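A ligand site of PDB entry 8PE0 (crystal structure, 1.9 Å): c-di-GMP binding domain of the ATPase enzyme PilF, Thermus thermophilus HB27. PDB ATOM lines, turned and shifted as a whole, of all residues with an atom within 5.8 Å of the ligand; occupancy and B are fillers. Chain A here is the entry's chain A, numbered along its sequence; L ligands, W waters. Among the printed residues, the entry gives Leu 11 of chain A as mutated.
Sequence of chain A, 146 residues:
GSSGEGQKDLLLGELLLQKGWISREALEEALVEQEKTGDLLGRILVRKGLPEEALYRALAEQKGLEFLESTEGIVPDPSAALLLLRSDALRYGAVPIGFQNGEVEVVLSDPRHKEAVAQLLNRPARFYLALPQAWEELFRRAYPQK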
ATOM      1  N   LEU A  10       7.730  29.272 -18.090  1.00  0.00           N
ATOM      2  CA  LEU A  10       7.422  28.606 -16.832  1.00  0.00           C
ATOM      3  C   LEU A  10       6.941  27.184 -17.077  1.00  0.00           C
ATOM      4  O   LEU A  10       6.280  26.897 -18.088  1.00  0.00           O
ATOM      5  CB  LEU A  10       6.369  29.407 -16.063  1.00  0.00           C
ATOM      6  CG  LEU A  10       6.877  30.265 -14.906  1.00  0.00           C
ATOM      7  CD1 LEU A  10       7.615  31.492 -15.408  1.00  0.00           C
ATOM      8  CD2 LEU A  10       5.723  30.666 -13.998  1.00  0.00           C
ATOM      9  N   LEU A  11       7.271  26.279 -16.156  1.00  0.00           N
ATOM     10  CA  LEU A  11       6.631  24.957 -16.161  1.00  0.00           C
ATOM     11  C   LEU A  11       5.159  25.055 -15.781  1.00  0.00           C
ATOM     12  O   LEU A  11       4.725  26.007 -15.116  1.00  0.00           O
ATOM     13  CB  LEU A  11       7.319  24.008 -15.179  1.00  0.00           C
ATOM     14  CG  LEU A  11       8.815  23.752 -15.403  1.00  0.00           C
ATOM     15  CD1 LEU A  11       9.452  23.311 -14.111  1.00  0.00           C
ATOM     16  CD2 LEU A  11       8.974  22.703 -16.490  1.00  0.00           C
ATOM     17  N   LEU A  12       4.380  24.037 -16.160  1.00  0.00           N
ATOM     18  CA  LEU A  12       2.950  24.035 -15.860  1.00  0.00           C
ATOM     19  C   LEU A  12       2.701  24.120 -14.353  1.00  0.00           C
ATOM     20  O   LEU A  12       1.857  24.899 -13.894  1.00  0.00           O
ATOM     21  CB  LEU A  12       2.286  22.794 -16.440  1.00  0.00           C
ATOM     22  CG  LEU A  12       0.856  22.525 -15.944  1.00  0.00           C
ATOM     23  CD1 LEU A  12      -0.105  23.576 -16.504  1.00  0.00           C
ATOM     24  CD2 LEU A  12       0.409  21.122 -16.374  1.00  0.00           C
ATOM     25  N   GLY A  13       3.429  23.325 -13.564  1.00  0.00           N
ATOM     26  CA  GLY A  13       3.267  23.367 -12.114  1.00  0.00           C
ATOM     27  C   GLY A  13       3.555  24.735 -11.537  1.00  0.00           C
ATOM     28  O   GLY A  13       2.775  25.262 -10.729  1.00  0.00           O
ATOM     29  N   GLU A  14       4.656  25.354 -11.980  1.00  0.00           N
ATOM     30  CA  GLU A  14       4.966  26.718 -11.555  1.00  0.00           C
ATOM     31  C   GLU A  14       3.833  27.681 -11.883  1.00  0.00           C
ATOM     32  O   GLU A  14       3.479  28.535 -11.061  1.00  0.00           O
ATOM     33  CB  GLU A  14       6.258  27.209 -12.200  1.00  0.00           C
ATOM     34  CG  GLU A  14       7.400  26.216 -12.223  1.00  0.00           C
ATOM     35  CD  GLU A  14       8.594  26.734 -13.032  1.00  0.00           C
ATOM     36  OE1 GLU A  14       9.583  27.179 -12.400  1.00  0.00           O
ATOM     37  OE2 GLU A  14       8.553  26.698 -14.283  1.00  0.00           O
ATOM     38  N   LEU A  17       0.915  27.154  -9.520  1.00  0.00           N
ATOM     39  CA  LEU A  17       1.240  27.604  -8.175  1.00  0.00           C
ATOM     40  C   LEU A  17       1.168  29.122  -8.086  1.00  0.00           C
ATOM     41  O   LEU A  17       0.628  29.670  -7.119  1.00  0.00           O
ATOM     42  CB  LEU A  17       2.640  27.129  -7.786  1.00  0.00           C
ATOM     43  CG  LEU A  17       2.812  25.690  -7.335  1.00  0.00           C
ATOM     44  CD1 LEU A  17       4.316  25.370  -7.234  1.00  0.00           C
ATOM     45  CD2 LEU A  17       2.124  25.462  -5.994  1.00  0.00           C
ATOM     46  N   LEU A  27       0.850  19.392  -6.010  1.00  0.00           N
ATOM     47  CA  LEU A  27       1.776  19.303  -7.135  1.00  0.00           C
ATOM     48  C   LEU A  27       2.862  18.266  -6.890  1.00  0.00           C
ATOM     49  O   LEU A  27       3.263  17.547  -7.814  1.00  0.00           O
ATOM     50  CB  LEU A  27       2.401  20.673  -7.423  1.00  0.00           C
ATOM     51  CG  LEU A  27       3.454  20.687  -8.535  1.00  0.00           C
ATOM     52  CD1 LEU A  27       2.869  20.244  -9.877  1.00  0.00           C
ATOM     53  CD2 LEU A  27       4.118  22.049  -8.675  1.00  0.00           C
ATOM     54  N   LEU A  31       3.727  14.946  -9.171  1.00  0.00           N
ATOM     55  CA  LEU A  31       5.033  14.721  -9.781  1.00  0.00           C
ATOM     56  C   LEU A  31       5.657  13.410  -9.328  1.00  0.00           C
ATOM     57  O   LEU A  31       6.444  12.807 -10.062  1.00  0.00           O
ATOM     58  CB  LEU A  31       5.972  15.886  -9.463  1.00  0.00           C
ATOM     59  CG  LEU A  31       5.691  17.223 -10.160  1.00  0.00           C
ATOM     60  CD1 LEU A  31       6.496  18.336  -9.496  1.00  0.00           C
ATOM     61  CD2 LEU A  31       5.983  17.150 -11.650  1.00  0.00           C
ATOM     62  N   GLN A  34       3.903  10.707 -11.272  1.00  0.00           N
ATOM     63  CA  GLN A  34       4.332  10.728 -12.680  1.00  0.00           C
ATOM     64  C   GLN A  34       5.677  10.032 -12.857  1.00  0.00           C
ATOM     65  O   GLN A  34       5.928   9.430 -13.905  1.00  0.00           O
ATOM     66  CB  GLN A  34       4.392  12.158 -13.191  1.00  0.00           C
ATOM     67  CG  GLN A  34       4.854  12.260 -14.636  1.00  0.00           C
ATOM     68  CD  GLN A  34       4.998  13.694 -15.114  1.00  0.00           C
ATOM     69  OE1 GLN A  34       5.805  14.459 -14.583  1.00  0.00           O
ATOM     70  NE2 GLN A  34       4.217  14.071 -16.118  1.00  0.00           N
ATOM     71  N   GLY A  38       4.423   7.971 -15.694  1.00  0.00           N
ATOM     72  CA  GLY A  38       4.652   8.621 -16.965  1.00  0.00           C
ATOM     73  C   GLY A  38       3.450   9.309 -17.564  1.00  0.00           C
ATOM     74  O   GLY A  38       3.540   9.761 -18.722  1.00  0.00           O
ATOM     75  N   ASP A  39       2.338   9.415 -16.835  1.00  0.00           N
ATOM     76  CA  ASP A  39       1.168  10.128 -17.339  1.00  0.00           C
ATOM     77  C   ASP A  39       1.437  11.621 -17.449  1.00  0.00           C
ATOM     78  O   ASP A  39       2.286  12.175 -16.741  1.00  0.00           O
ATOM     79  CB  ASP A  39      -0.044   9.895 -16.432  1.00  0.00           C
ATOM     80  CG  ASP A  39      -0.828   8.641 -16.779  1.00  0.00           C
ATOM     81  OD1 ASP A  39      -0.229   7.680 -17.317  1.00  0.00           O
ATOM     82  OD2 ASP A  39      -2.046   8.610 -16.506  1.00  0.00           O
ATOM     83  N   LEU A  40       0.706  12.280 -18.352  1.00  0.00           N
ATOM     84  CA  LEU A  40       0.778  13.732 -18.483  1.00  0.00           C
ATOM     85  C   LEU A  40       0.441  14.397 -17.159  1.00  0.00           C
ATOM     86  O   LEU A  40      -0.478  13.970 -16.451  1.00  0.00           O
ATOM     87  CB  LEU A  40      -0.199  14.198 -19.564  1.00  0.00           C
ATOM     88  CG  LEU A  40       0.227  14.638 -20.942  1.00  0.00           C
ATOM     89  CD1 LEU A  40      -0.994  15.274 -21.578  1.00  0.00           C
ATOM     90  CD2 LEU A  40       1.419  15.595 -20.939  1.00  0.00           C
ATOM     91  N   LEU A  41       1.197  15.437 -16.809  1.00  0.00           N
ATOM     92  CA  LEU A  41       1.033  16.020 -15.476  1.00  0.00           C
ATOM     93  C   LEU A  41      -0.357  16.615 -15.300  1.00  0.00           C
ATOM     94  O   LEU A  41      -0.988  16.418 -14.247  1.00  0.00           O
ATOM     95  CB  LEU A  41       2.094  17.086 -15.235  1.00  0.00           C
ATOM     96  CG  LEU A  41       1.934  17.773 -13.868  1.00  0.00           C
ATOM     97  CD1 LEU A  41       2.023  16.746 -12.758  1.00  0.00           C
ATOM     98  CD2 LEU A  41       2.941  18.889 -13.655  1.00  0.00           C
ATOM     99  N   GLY A  42      -0.855  17.352 -16.308  1.00  0.00           N
ATOM    100  CA  GLY A  42      -2.169  17.960 -16.149  1.00  0.00           C
ATOM    101  C   GLY A  42      -3.274  16.921 -16.026  1.00  0.00           C
ATOM    102  O   GLY A  42      -4.283  17.158 -15.373  1.00  0.00           O
ATOM    103  N   ARG A  43      -3.083  15.754 -16.637  1.00  0.00           N
ATOM    104  CA  ARG A  43      -4.056  14.679 -16.483  1.00  0.00           C
ATOM    105  C   ARG A  43      -4.080  14.172 -15.048  1.00  0.00           C
ATOM    106  O   ARG A  43      -5.151  13.881 -14.503  1.00  0.00           O
ATOM    107  CB  ARG A  43      -3.730  13.549 -17.461  1.00  0.00           C
ATOM    108  CG  ARG A  43      -4.807  12.482 -17.570  1.00  0.00           C
ATOM    109  N   LEU A  55      -6.510  24.031 -15.734  1.00  0.00           N
ATOM    110  CA  LEU A  55      -5.440  23.447 -16.535  1.00  0.00           C
ATOM    111  C   LEU A  55      -5.313  24.170 -17.881  1.00  0.00           C
ATOM    112  O   LEU A  55      -4.219  24.567 -18.282  1.00  0.00           O
ATOM    113  CB  LEU A  55      -5.706  21.954 -16.746  1.00  0.00           C
ATOM    114  CG  LEU A  55      -4.702  21.246 -17.666  1.00  0.00           C
ATOM    115  CD1 LEU A  55      -3.314  21.362 -17.074  1.00  0.00           C
ATOM    116  CD2 LEU A  55      -5.070  19.776 -17.869  1.00  0.00           C
ATOM    117  N   TYR A  56      -6.431  24.364 -18.583  1.00  0.00           N
ATOM    118  CA  TYR A  56      -6.325  24.926 -19.929  1.00  0.00           C
ATOM    119  C   TYR A  56      -5.932  26.399 -19.899  1.00  0.00           C
ATOM    120  O   TYR A  56      -5.186  26.861 -20.765  1.00  0.00           O
ATOM    121  CB  TYR A  56      -7.638  24.739 -20.695  1.00  0.00           C
ATOM    122  CG  TYR A  56      -7.655  23.421 -21.440  1.00  0.00           C
ATOM    123  CD1 TYR A  56      -7.583  22.223 -20.742  1.00  0.00           C
ATOM    124  CD2 TYR A  56      -7.752  23.380 -22.827  1.00  0.00           C
ATOM    125  CE1 TYR A  56      -7.597  21.004 -21.402  1.00  0.00           C
ATOM    126  CE2 TYR A  56      -7.785  22.169 -23.506  1.00  0.00           C
ATOM    127  CZ  TYR A  56      -7.694  20.986 -22.790  1.00  0.00           C
ATOM    128  OH  TYR A  56      -7.702  19.775 -23.441  1.00  0.00           O
ATOM    129  N   LEU A  59      -2.188  26.328 -19.461  1.00  0.00           N
ATOM    130  CA  LEU A  59      -1.475  25.890 -20.660  1.00  0.00           C
ATOM    131  C   LEU A  59      -1.567  26.932 -21.761  1.00  0.00           C
ATOM    132  O   LEU A  59      -0.648  27.062 -22.575  1.00  0.00           O
ATOM    133  CB  LEU A  59      -2.028  24.551 -21.154  1.00  0.00           C
ATOM    134  CG  LEU A  59      -1.801  23.322 -20.248  1.00  0.00           C
ATOM    135  CD1 LEU A  59      -2.679  22.151 -20.641  1.00  0.00           C
ATOM    136  CD2 LEU A  59      -0.367  22.919 -20.337  1.00  0.00           C
ATOM    137  N   GLN A  62       1.026  29.510 -21.093  1.00  0.00           N
ATOM    138  CA  GLN A  62       2.380  28.978 -21.299  1.00  0.00           C
ATOM    139  C   GLN A  62       2.778  29.010 -22.764  1.00  0.00           C
ATOM    140  O   GLN A  62       3.956  29.220 -23.073  1.00  0.00           O
ATOM    141  CB  GLN A  62       2.462  27.552 -20.761  1.00  0.00           C
ATOM    142  CG  GLN A  62       3.833  26.917 -20.873  1.00  0.00           C
ATOM    143  CD  GLN A  62       3.823  25.461 -20.446  1.00  0.00           C
ATOM    144  OE1 GLN A  62       3.215  24.617 -21.111  1.00  0.00           O
ATOM    145  NE2 GLN A  62       4.487  25.171 -19.335  1.00  0.00           N
ATOM    146  N   LYS A  63       1.835  28.822 -23.665  1.00  0.00           N
ATOM    147  CA  LYS A  63       2.120  28.771 -25.095  1.00  0.00           C
ATOM    148  C   LYS A  63       1.678  30.031 -25.844  1.00  0.00           C
ATOM    149  O   LYS A  63       1.728  30.051 -27.076  1.00  0.00           O
ATOM    150  CB  LYS A  63       1.469  27.541 -25.727  1.00  0.00           C
ATOM    151  CG  LYS A  63       1.849  26.223 -25.091  1.00  0.00           C
ATOM    152  CD  LYS A  63       3.216  25.703 -25.561  1.00  0.00           C
ATOM    153  CE  LYS A  63       3.449  24.282 -25.047  1.00  0.00           C
ATOM    154  NZ  LYS A  63       4.645  23.593 -25.633  1.00  0.00           N
ATOM    155  N   SER A 109      -7.146  22.479 -30.065  1.00  0.00           N
ATOM    156  CA  SER A 109      -7.668  21.637 -29.009  1.00  0.00           C
ATOM    157  C   SER A 109      -6.599  21.201 -28.018  1.00  0.00           C
ATOM    158  O   SER A 109      -6.939  20.743 -26.928  1.00  0.00           O
ATOM    159  CB  SER A 109      -8.315  20.387 -29.590  1.00  0.00           C
ATOM    160  OG  SER A 109      -7.293  19.568 -30.143  1.00  0.00           O
ATOM    161  N   ASP A 110      -5.319  21.351 -28.363  1.00  0.00           N
ATOM    162  CA  ASP A 110      -4.186  20.944 -27.530  1.00  0.00           C
ATOM    163  C   ASP A 110      -3.056  21.937 -27.744  1.00  0.00           C
ATOM    164  O   ASP A 110      -2.493  22.017 -28.845  1.00  0.00           O
ATOM    165  CB  ASP A 110      -3.766  19.525 -27.898  1.00  0.00           C
ATOM    166  CG  ASP A 110      -2.716  18.936 -26.938  1.00  0.00           C
ATOM    167  OD1 ASP A 110      -1.913  19.687 -26.345  1.00  0.00           O
ATOM    168  OD2 ASP A 110      -2.693  17.696 -26.806  1.00  0.00           O
ATOM    169  N   PRO A 111      -2.695  22.713 -26.721  1.00  0.00           N
ATOM    170  CA  PRO A 111      -1.594  23.669 -26.890  1.00  0.00           C
ATOM    171  C   PRO A 111      -0.273  23.041 -27.319  1.00  0.00           C
ATOM    172  O   PRO A 111       0.569  23.744 -27.894  1.00  0.00           O
ATOM    173  CB  PRO A 111      -1.466  24.292 -25.485  1.00  0.00           C
ATOM    174  CG  PRO A 111      -2.003  23.236 -24.568  1.00  0.00           C
ATOM    175  CD  PRO A 111      -3.151  22.625 -25.327  1.00  0.00           C
ATOM    176  N   ARG A 112      -0.071  21.737 -27.070  1.00  0.00           N
ATOM    177  CA  ARG A 112       1.191  21.129 -27.505  1.00  0.00           C
ATOM    178  C   ARG A 112       1.325  21.084 -29.023  1.00  0.00           C
ATOM    179  O   ARG A 112       2.429  20.856 -29.524  1.00  0.00           O
ATOM    180  CB  ARG A 112       1.324  19.710 -26.962  1.00  0.00           C
ATOM    181  CG  ARG A 112       1.536  19.632 -25.429  1.00  0.00           C
ATOM    182  CD  ARG A 112       1.501  18.170 -24.979  1.00  0.00           C
ATOM    183  NE  ARG A 112       0.159  17.622 -25.171  1.00  0.00           N
ATOM    184  CZ  ARG A 112      -0.147  16.331 -25.077  1.00  0.00           C
ATOM    185  NH1 ARG A 112       0.789  15.450 -24.785  1.00  0.00           N
ATOM    186  NH2 ARG A 112      -1.389  15.921 -25.275  1.00  0.00           N
HETATM  187  P1  LIG L   1       4.731  16.425 -18.960  1.00  0.00           P
HETATM  188  O1  LIG L   1       3.766  16.039 -17.867  1.00  0.00           O
HETATM  189  O2  LIG L   1       4.931  15.196 -19.790  1.00  0.00           O
HETATM  190  O3  LIG L   1       4.118  17.512 -19.985  1.00  0.00           O
HETATM  191  C1  LIG L   1       4.907  17.839 -21.150  1.00  0.00           C
HETATM  192  C2  LIG L   1       4.288  19.203 -21.626  1.00  0.00           C
HETATM  193  O4  LIG L   1       3.035  19.008 -21.914  1.00  0.00           O
HETATM  194  C3  LIG L   1       4.304  20.207 -20.472  1.00  0.00           C
HETATM  195  O5  LIG L   1       5.361  21.009 -20.699  1.00  0.00           O
HETATM  196  C4  LIG L   1       3.002  21.017 -20.636  1.00  0.00           C
HETATM  197  O6  LIG L   1       3.283  22.063 -21.691  1.00  0.00           O
HETATM  198  C5  LIG L   1       2.215  20.217 -21.278  1.00  0.00           C
HETATM  199  N1  LIG L   1       1.026  19.592 -20.706  1.00  0.00           N
HETATM  200  C6  LIG L   1       1.356  19.181 -19.448  1.00  0.00           C
HETATM  201  N2  LIG L   1       0.230  18.551 -18.921  1.00  0.00           N
HETATM  202  C7  LIG L   1      -0.730  18.584 -19.881  1.00  0.00           C
HETATM  203  C8  LIG L   1      -2.167  18.112 -20.068  1.00  0.00           C
HETATM  204  O7  LIG L   1      -2.748  17.534 -19.212  1.00  0.00           O
HETATM  205  N3  LIG L   1      -2.827  18.341 -21.307  1.00  0.00           N
HETATM  206  C9  LIG L   1      -2.171  19.037 -22.398  1.00  0.00           C
HETATM  207  N4  LIG L   1      -2.795  19.269 -23.640  1.00  0.00           N
HETATM  208  N5  LIG L   1      -0.832  19.481 -22.240  1.00  0.00           N
HETATM  209  C10 LIG L   1      -0.179  19.214 -20.959  1.00  0.00           C
HETATM  210  P2  LIG L   1       6.023  21.683 -19.266  1.00  0.00           P
HETATM  211  O8  LIG L   1       5.042  22.527 -18.466  1.00  0.00           O
HETATM  212  O9  LIG L   1       7.176  22.552 -19.667  1.00  0.00           O
HETATM  213  O10 LIG L   1       6.487  20.263 -18.381  1.00  0.00           O
HETATM  214  C11 LIG L   1       7.785  19.737 -18.613  1.00  0.00           C
HETATM  215  C12 LIG L   1       7.904  18.612 -17.621  1.00  0.00           C
HETATM  216  O11 LIG L   1       8.323  19.004 -16.442  1.00  0.00           O
HETATM  217  C13 LIG L   1       6.397  17.910 -17.398  1.00  0.00           C
HETATM  218  O12 LIG L   1       6.341  16.779 -18.431  1.00  0.00           O
HETATM  219  C14 LIG L   1       6.407  17.471 -16.230  1.00  0.00           C
HETATM  220  O13 LIG L   1       7.071  16.110 -16.160  1.00  0.00           O
HETATM  221  C15 LIG L   1       7.362  18.485 -15.393  1.00  0.00           C
HETATM  222  N6  LIG L   1       6.733  19.512 -14.826  1.00  0.00           N
HETATM  223  C16 LIG L   1       5.653  20.284 -15.169  1.00  0.00           C
HETATM  224  N7  LIG L   1       5.488  21.232 -14.197  1.00  0.00           N
HETATM  225  C17 LIG L   1       6.467  21.034 -13.281  1.00  0.00           C
HETATM  226  C18 LIG L   1       6.834  21.767 -11.974  1.00  0.00           C
HETATM  227  O14 LIG L   1       6.209  22.680 -11.602  1.00  0.00           O
HETATM  228  N8  LIG L   1       7.947  21.332 -11.188  1.00  0.00           N
HETATM  229  C19 LIG L   1       8.749  20.210 -11.626  1.00  0.00           C
HETATM  230  N9  LIG L   1       9.919  19.770 -10.805  1.00  0.00           N
HETATM  231  N10 LIG L   1       8.402  19.506 -12.876  1.00  0.00           N
HETATM  232  C20 LIG L   1       7.234  19.970 -13.688  1.00  0.00           C
HETATM  233  O   HOH W   1      -5.464  16.447 -19.442  1.00  0.00           O
HETATM  234  O   HOH W   2       7.320  15.404 -21.858  1.00  0.00           O
HETATM  235  O   HOH W   3       6.268  21.455 -23.439  1.00  0.00           O
HETATM  236  O   HOH W   4       7.821  25.614 -20.706  1.00  0.00           O
HETATM  237  O   HOH W   5      12.206  18.409  -9.777  1.00  0.00           O
HETATM  238  O   HOH W   6       8.462  22.364  -8.724  1.00  0.00           O
HETATM  239  O   HOH W   7      -5.562  19.377 -24.590  1.00  0.00           O
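Leu 11 touches the ligand (CB to N7, 3.5 Å). Leu 27 touches the ligand (CD2 to O14, 3.7 Å). CD2 of Leu 31 touches N10 of the ligand, 3.6 Å away. Leu 40 touches the ligand (CD1 to C8, 3.4 Å). CD2 of Leu 55 touches O7 of the ligand (3.5 Å). Leu 59 touches the ligand. Pro 111 touches the ligand (CD to N4, 3.8 Å). CD of Arg 112 touches O4 of the ligand, at 3.5 Å. Hydrophobic or aromatic side chains that line the ligand: Leu 11, Leu 12, Leu 27, Leu 31, Leu 40, Leu 41, Leu 55, Leu 59 and Pro 111. Of the 24 residues printed, 17 come within 4 Å of the ligand. The nearest printed residue that does not touch the ligand is Lys 63 (4.03 Å).
Water W3 bridges O5 of the ligand (2.9 Å) and NZ of Lys 63 (3.5 Å). Water W7 lies within hydrogen-bond range of OH of Tyr 56 (2.5 Å), N4 of the ligand (2.9 Å) and O of Ser 109 (3.0 Å). Water W4 lies within hydrogen-bond range of an oxygen (O9) of the ligand (3.3 Å) and the backbone carbonyl oxygen of Leu 10 (3.3 Å).
OD2 of Asp 110 is in salt-bridge range of NH2 of Arg 112 (2.7 Å). O of Leu 10 is in hydrogen-bond range of NE2 of Gln 62. NE2 of Gln 34 sits at hydrogen-bond distance from O of Asp 39 (2.8 Å). The backbone NH (N) of Leu 41 lies close to the side-chain amide nitrogen (NE2) of Gln 34 (3.4 Å). The backbone NH (N) of Leu 12 sits close to the side-chain amide nitrogen (NE2) of Gln 62.
OD1 of Asp 110 is in hydrogen-bond range of N4 of the ligand. The side-chain amide oxygen (OE1) of Gln 62 is in hydrogen-bond range of an oxygen (O6) of the ligand. The backbone NH of Leu 41 lies within hydrogen-bond range of an oxygen (O1) of the ligand (2.8 Å). The backbone NH of Leu 12 sits at hydrogen-bond distance from an oxygen (O8) of the ligand (2.8 Å). The backbone NH (N) of Gly 42 lies within hydrogen-bond range of a nitrogen (N2) of the ligand, at 3.1 Å. The backbone NH of Arg 43 lies within hydrogen-bond range of an oxygen (O7) of the ligand (3.1 Å). The backbone NH of Glu 14 lies within hydrogen-bond range of an oxygen (O14) of the ligand. OE1 of Gln 34 is in hydrogen-bond range of O13 of the ligand (2.6 Å). N of Gly 13 sits at hydrogen-bond distance from N7 of the ligand, 3.0 Å away.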
